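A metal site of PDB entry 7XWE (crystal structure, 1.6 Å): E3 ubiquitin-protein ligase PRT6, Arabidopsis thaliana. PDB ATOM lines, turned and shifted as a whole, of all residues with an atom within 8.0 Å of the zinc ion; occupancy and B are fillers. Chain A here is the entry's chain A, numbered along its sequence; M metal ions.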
ATOM      1  N   ARG A  21     -26.554   4.666  22.394  1.00  0.00           N
ATOM      2  CA  ARG A  21     -25.423   5.451  22.855  1.00  0.00           C
ATOM      3  C   ARG A  21     -25.401   5.328  24.369  1.00  0.00           C
ATOM      4  O   ARG A  21     -26.434   5.456  25.021  1.00  0.00           O
ATOM      5  CB  ARG A  21     -25.542   6.918  22.432  1.00  0.00           C
ATOM      6  CG  ARG A  21     -24.395   7.741  22.950  1.00  0.00           C
ATOM      7  CD  ARG A  21     -24.298   9.136  22.343  1.00  0.00           C
ATOM      8  NE  ARG A  21     -23.146   9.782  22.919  1.00  0.00           N
ATOM      9  CZ  ARG A  21     -22.991  11.098  23.059  1.00  0.00           C
ATOM     10  NH1 ARG A  21     -23.954  11.913  22.657  1.00  0.00           N
ATOM     11  NH2 ARG A  21     -21.891  11.557  23.629  1.00  0.00           N
ATOM     12  N   CYS A  22     -24.228   5.059  24.940  1.00  0.00           N
ATOM     13  CA  CYS A  22     -24.069   5.085  26.395  1.00  0.00           C
ATOM     14  C   CYS A  22     -22.902   5.988  26.741  1.00  0.00           C
ATOM     15  O   CYS A  22     -21.745   5.634  26.516  1.00  0.00           O
ATOM     16  CB  CYS A  22     -23.860   3.690  27.009  1.00  0.00           C
ATOM     17  SG  CYS A  22     -23.781   3.902  28.805  1.00  0.00           S
ATOM     18  N   ARG A  23     -23.216   7.160  27.287  1.00  0.00           N
ATOM     19  CA  ARG A  23     -22.154   8.126  27.556  1.00  0.00           C
ATOM     20  C   ARG A  23     -21.234   7.677  28.677  1.00  0.00           C
ATOM     21  O   ARG A  23     -20.098   8.144  28.766  1.00  0.00           O
ATOM     22  CB  ARG A  23     -22.792   9.468  27.881  1.00  0.00           C
ATOM     23  CG  ARG A  23     -23.535  10.039  26.692  1.00  0.00           C
ATOM     24  CD  ARG A  23     -24.516  11.096  27.145  1.00  0.00           C
ATOM     25  NE  ARG A  23     -25.372  11.564  26.047  1.00  0.00           N
ATOM     26  CZ  ARG A  23     -26.467  10.931  25.630  1.00  0.00           C
ATOM     27  NH1 ARG A  23     -26.872   9.800  26.192  1.00  0.00           N
ATOM     28  NH2 ARG A  23     -27.178  11.459  24.646  1.00  0.00           N
ATOM     29  N   THR A  24     -21.717   6.786  29.534  1.00  0.00           N
ATOM     30  CA  THR A  24     -20.888   6.275  30.624  1.00  0.00           C
ATOM     31  C   THR A  24     -19.827   5.311  30.105  1.00  0.00           C
ATOM     32  O   THR A  24     -18.701   5.281  30.605  1.00  0.00           O
ATOM     33  CB  THR A  24     -21.798   5.597  31.643  1.00  0.00           C
ATOM     34  OG1 THR A  24     -22.836   6.491  32.055  1.00  0.00           O
ATOM     35  CG2 THR A  24     -20.999   5.172  32.866  1.00  0.00           C
ATOM     36  N   CYS A  25     -20.173   4.532  29.072  1.00  0.00           N
ATOM     37  CA  CYS A  25     -19.332   3.454  28.583  1.00  0.00           C
ATOM     38  C   CYS A  25     -18.521   3.816  27.351  1.00  0.00           C
ATOM     39  O   CYS A  25     -17.534   3.133  27.063  1.00  0.00           O
ATOM     40  CB  CYS A  25     -20.184   2.243  28.233  1.00  0.00           C
ATOM     41  SG  CYS A  25     -20.896   1.379  29.640  1.00  0.00           S
ATOM     42  N   GLU A  26     -18.930   4.824  26.590  1.00  0.00           N
ATOM     43  CA  GLU A  26     -18.307   5.084  25.293  1.00  0.00           C
ATOM     44  C   GLU A  26     -16.862   5.565  25.466  1.00  0.00           C
ATOM     45  O   GLU A  26     -16.546   6.286  26.415  1.00  0.00           O
ATOM     46  CB  GLU A  26     -19.123   6.117  24.518  1.00  0.00           C
ATOM     47  CG  GLU A  26     -19.070   7.525  25.096  1.00  0.00           C
ATOM     48  CD  GLU A  26     -20.039   8.487  24.445  1.00  0.00           C
ATOM     49  OE1 GLU A  26     -21.019   8.037  23.821  1.00  0.00           O
ATOM     50  OE2 GLU A  26     -19.806   9.716  24.572  1.00  0.00           O
ATOM     51  N   ILE A  33     -23.497   0.738  20.698  1.00  0.00           N
ATOM     52  CA  ILE A  33     -23.634  -0.726  20.732  1.00  0.00           C
ATOM     53  C   ILE A  33     -25.038  -1.108  20.306  1.00  0.00           C
ATOM     54  O   ILE A  33     -26.004  -0.356  20.498  1.00  0.00           O
ATOM     55  CB  ILE A  33     -23.305  -1.356  22.107  1.00  0.00           C
ATOM     56  CG1 ILE A  33     -24.209  -0.820  23.217  1.00  0.00           C
ATOM     57  CG2 ILE A  33     -21.794  -1.133  22.446  1.00  0.00           C
ATOM     58  CD1 ILE A  33     -24.066  -1.622  24.530  1.00  0.00           C
ATOM     59  N   PHE A  38     -26.721  -4.140  24.261  1.00  0.00           N
ATOM     60  CA  PHE A  38     -27.161  -3.285  25.355  1.00  0.00           C
ATOM     61  C   PHE A  38     -28.017  -4.073  26.329  1.00  0.00           C
ATOM     62  O   PHE A  38     -27.818  -3.998  27.547  1.00  0.00           O
ATOM     63  CB  PHE A  38     -27.954  -2.085  24.829  1.00  0.00           C
ATOM     64  CG  PHE A  38     -28.410  -1.159  25.922  1.00  0.00           C
ATOM     65  CD1 PHE A  38     -27.538  -0.194  26.426  1.00  0.00           C
ATOM     66  CD2 PHE A  38     -29.654  -1.286  26.462  1.00  0.00           C
ATOM     67  CE1 PHE A  38     -27.931   0.647  27.439  1.00  0.00           C
ATOM     68  CE2 PHE A  38     -30.065  -0.445  27.461  1.00  0.00           C
ATOM     69  CZ  PHE A  38     -29.193   0.521  27.965  1.00  0.00           C
ATOM     70  N   GLY A  41     -26.140  -6.403  28.728  1.00  0.00           N
ATOM     71  CA  GLY A  41     -25.124  -5.815  29.573  1.00  0.00           C
ATOM     72  C   GLY A  41     -25.734  -5.066  30.758  1.00  0.00           C
ATOM     73  O   GLY A  41     -26.943  -5.089  30.982  1.00  0.00           O
ATOM     74  N   ASP A  42     -24.849  -4.425  31.514  1.00  0.00           N
ATOM     75  CA  ASP A  42     -25.216  -3.693  32.725  1.00  0.00           C
ATOM     76  C   ASP A  42     -24.944  -2.204  32.498  1.00  0.00           C
ATOM     77  O   ASP A  42     -23.798  -1.749  32.532  1.00  0.00           O
ATOM     78  CB  ASP A  42     -24.426  -4.198  33.935  1.00  0.00           C
ATOM     79  CG  ASP A  42     -24.572  -3.295  35.164  1.00  0.00           C
ATOM     80  OD1 ASP A  42     -23.837  -3.530  36.153  1.00  0.00           O
ATOM     81  OD2 ASP A  42     -25.405  -2.362  35.163  1.00  0.00           O
ATOM     82  N   HIS A  43     -26.019  -1.457  32.275  1.00  0.00           N
ATOM     83  CA  HIS A  43     -25.955  -0.014  32.144  1.00  0.00           C
ATOM     84  C   HIS A  43     -26.878   0.637  33.155  1.00  0.00           C
ATOM     85  O   HIS A  43     -27.401   1.711  32.922  1.00  0.00           O
ATOM     86  CB  HIS A  43     -26.285   0.387  30.715  1.00  0.00           C
ATOM     87  CG  HIS A  43     -25.363  -0.276  29.738  1.00  0.00           C
ATOM     88  ND1 HIS A  43     -24.117   0.229  29.441  1.00  0.00           N
ATOM     89  CD2 HIS A  43     -25.465  -1.453  29.078  1.00  0.00           C
ATOM     90  CE1 HIS A  43     -23.512  -0.582  28.597  1.00  0.00           C
ATOM     91  NE2 HIS A  43     -24.313  -1.602  28.348  1.00  0.00           N
ATOM     92  N   ASN A  44     -27.064   0.015  34.319  1.00  0.00           N
ATOM     93  CA  ASN A  44     -27.913   0.647  35.314  1.00  0.00           C
ATOM     94  C   ASN A  44     -27.271   1.939  35.806  1.00  0.00           C
ATOM     95  O   ASN A  44     -26.083   1.984  36.125  1.00  0.00           O
ATOM     96  CB  ASN A  44     -28.200  -0.301  36.465  1.00  0.00           C
ATOM     97  CG  ASN A  44     -28.882  -1.570  36.012  1.00  0.00           C
ATOM     98  OD1 ASN A  44     -29.868  -1.539  35.281  1.00  0.00           O
ATOM     99  ND2 ASN A  44     -28.354  -2.685  36.455  1.00  0.00           N
ATOM    100  N   SER A  45     -28.077   2.992  35.820  1.00  0.00           N
ATOM    101  CA  SER A  45     -27.710   4.375  36.148  1.00  0.00           C
ATOM    102  C   SER A  45     -26.732   4.994  35.161  1.00  0.00           C
ATOM    103  O   SER A  45     -26.209   6.082  35.411  1.00  0.00           O
ATOM    104  CB  SER A  45     -27.158   4.492  37.577  1.00  0.00           C
ATOM    105  OG  SER A  45     -28.216   4.327  38.531  1.00  0.00           O
ATOM    106  N   HIS A  46     -26.473   4.342  34.029  1.00  0.00           N
ATOM    107  CA  HIS A  46     -25.661   5.004  33.030  1.00  0.00           C
ATOM    108  C   HIS A  46     -26.490   6.002  32.239  1.00  0.00           C
ATOM    109  O   HIS A  46     -27.709   5.902  32.167  1.00  0.00           O
ATOM    110  CB  HIS A  46     -25.096   4.014  32.029  1.00  0.00           C
ATOM    111  CG  HIS A  46     -24.133   3.049  32.622  1.00  0.00           C
ATOM    112  ND1 HIS A  46     -23.346   2.226  31.852  1.00  0.00           N
ATOM    113  CD2 HIS A  46     -23.831   2.779  33.908  1.00  0.00           C
ATOM    114  CE1 HIS A  46     -22.598   1.489  32.645  1.00  0.00           C
ATOM    115  NE2 HIS A  46     -22.867   1.807  33.892  1.00  0.00           N
ATOM    116  N   ASP A  47     -25.797   6.934  31.569  1.00  0.00           N
ATOM    117  CA  ASP A  47     -26.504   7.954  30.800  1.00  0.00           C
ATOM    118  C   ASP A  47     -26.572   7.532  29.337  1.00  0.00           C
ATOM    119  O   ASP A  47     -25.761   7.929  28.501  1.00  0.00           O
ATOM    120  CB  ASP A  47     -25.827   9.314  30.956  1.00  0.00           C
ATOM    121  CG  ASP A  47     -26.582  10.419  30.265  1.00  0.00           C
ATOM    122  OD1 ASP A  47     -27.696  10.149  29.764  1.00  0.00           O
ATOM    123  OD2 ASP A  47     -26.066  11.536  30.270  1.00  0.00           O
ATOM    124  N   TYR A  48     -27.552   6.670  29.036  1.00  0.00           N
ATOM    125  CA  TYR A  48     -27.728   6.078  27.708  1.00  0.00           C
ATOM    126  C   TYR A  48     -28.977   6.626  27.020  1.00  0.00           C
ATOM    127  O   TYR A  48     -29.893   7.162  27.661  1.00  0.00           O
ATOM    128  CB  TYR A  48     -27.772   4.540  27.803  1.00  0.00           C
ATOM    129  CG  TYR A  48     -28.899   3.981  28.641  1.00  0.00           C
ATOM    130  CD1 TYR A  48     -30.186   3.914  28.136  1.00  0.00           C
ATOM    131  CD2 TYR A  48     -28.687   3.526  29.945  1.00  0.00           C
ATOM    132  CE1 TYR A  48     -31.245   3.428  28.897  1.00  0.00           C
ATOM    133  CE2 TYR A  48     -29.729   3.046  30.715  1.00  0.00           C
ATOM    134  CZ  TYR A  48     -31.010   2.988  30.167  1.00  0.00           C
ATOM    135  OH  TYR A  48     -32.075   2.495  30.900  1.00  0.00           O
ATOM    136  N   TRP A  66     -15.033   1.001  23.689  1.00  0.00           N
ATOM    137  CA  TRP A  66     -16.082   0.818  24.688  1.00  0.00           C
ATOM    138  C   TRP A  66     -15.439   0.262  25.945  1.00  0.00           C
ATOM    139  O   TRP A  66     -14.562  -0.599  25.852  1.00  0.00           O
ATOM    140  CB  TRP A  66     -17.121  -0.175  24.159  1.00  0.00           C
ATOM    141  CG  TRP A  66     -18.467  -0.139  24.773  1.00  0.00           C
ATOM    142  CD1 TRP A  66     -18.961  -0.978  25.729  1.00  0.00           C
ATOM    143  CD2 TRP A  66     -19.525   0.756  24.446  1.00  0.00           C
ATOM    144  NE1 TRP A  66     -20.258  -0.658  26.023  1.00  0.00           N
ATOM    145  CE2 TRP A  66     -20.628   0.416  25.250  1.00  0.00           C
ATOM    146  CE3 TRP A  66     -19.632   1.839  23.571  1.00  0.00           C
ATOM    147  CZ2 TRP A  66     -21.831   1.102  25.165  1.00  0.00           C
ATOM    148  CZ3 TRP A  66     -20.810   2.518  23.509  1.00  0.00           C
ATOM    149  CH2 TRP A  66     -21.904   2.145  24.299  1.00  0.00           C
ATOM    150  N   LYS A  67     -15.849   0.786  27.099  1.00  0.00           N
ATOM    151  CA  LYS A  67     -15.288   0.331  28.371  1.00  0.00           C
ATOM    152  C   LYS A  67     -15.674  -1.120  28.629  1.00  0.00           C
ATOM    153  O   LYS A  67     -16.847  -1.484  28.462  1.00  0.00           O
ATOM    154  CB  LYS A  67     -15.742   1.252  29.512  1.00  0.00           C
ATOM    155  CG  LYS A  67     -15.196   2.696  29.462  1.00  0.00           C
ATOM    156  CD  LYS A  67     -15.833   3.596  30.534  1.00  0.00           C
ATOM    157  CE  LYS A  67     -15.734   5.100  30.237  1.00  0.00           C
ATOM    158  NZ  LYS A  67     -14.746   5.415  29.208  1.00  0.00           N
ATOM    159  N   ASP A  69     -16.352  -2.858  31.271  1.00  0.00           N
ATOM    160  CA  ASP A  69     -17.443  -3.159  32.186  1.00  0.00           C
ATOM    161  C   ASP A  69     -18.822  -2.905  31.539  1.00  0.00           C
ATOM    162  O   ASP A  69     -19.842  -3.309  32.112  1.00  0.00           O
ATOM    163  CB  ASP A  69     -17.252  -2.334  33.465  1.00  0.00           C
ATOM    164  CG  ASP A  69     -15.978  -2.750  34.259  1.00  0.00           C
ATOM    165  OD1 ASP A  69     -15.368  -3.825  34.013  1.00  0.00           O
ATOM    166  OD2 ASP A  69     -15.574  -1.973  35.156  1.00  0.00           O
ATOM    167  N   GLY A  70     -18.853  -2.302  30.350  1.00  0.00           N
ATOM    168  CA  GLY A  70     -20.028  -2.136  29.533  1.00  0.00           C
ATOM    169  C   GLY A  70     -20.197  -3.162  28.437  1.00  0.00           C
ATOM    170  O   GLY A  70     -21.139  -3.040  27.641  1.00  0.00           O
ATOM    171  N   PHE A  71     -19.305  -4.144  28.360  1.00  0.00           N
ATOM    172  CA  PHE A  71     -19.461  -5.256  27.424  1.00  0.00           C
ATOM    173  C   PHE A  71     -20.662  -6.094  27.849  1.00  0.00           C
ATOM    174  O   PHE A  71     -20.937  -6.249  29.035  1.00  0.00           O
ATOM    175  CB  PHE A  71     -18.221  -6.156  27.418  1.00  0.00           C
ATOM    176  CG  PHE A  71     -16.968  -5.537  26.804  1.00  0.00           C
ATOM    177  CD1 PHE A  71     -15.767  -6.211  26.907  1.00  0.00           C
ATOM    178  CD2 PHE A  71     -16.985  -4.321  26.138  1.00  0.00           C
ATOM    179  CE1 PHE A  71     -14.605  -5.675  26.374  1.00  0.00           C
ATOM    180  CE2 PHE A  71     -15.817  -3.798  25.604  1.00  0.00           C
ATOM    181  CZ  PHE A  71     -14.638  -4.474  25.706  1.00  0.00           C
HETATM  182 ZN    ZN M   1     -23.087   1.974  29.818  1.00  0.00          ZN
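O of Cys 25 lies within hydrogen-bond range of N of Lys 67 (2.9 Å). The side-chain sulfur of Cys 22 sits close to the backbone NH of Thr 24, 3.6 Å away.
Four residues have an atom within 4 Å of the zinc ion: Cys 22, Cys 25, His 43 and His 46.
ND1 of His 43 is bound to the zinc ion, 2.1 Å away. The zinc ion is bound by ND1 of His 46 (2.1 Å). SG of Cys 25 binds the zinc ion, 2.3 Å away. SG of Cys 22 binds the zinc ion (2.3 Å). The zinc ion has four donor atoms within binding distance.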
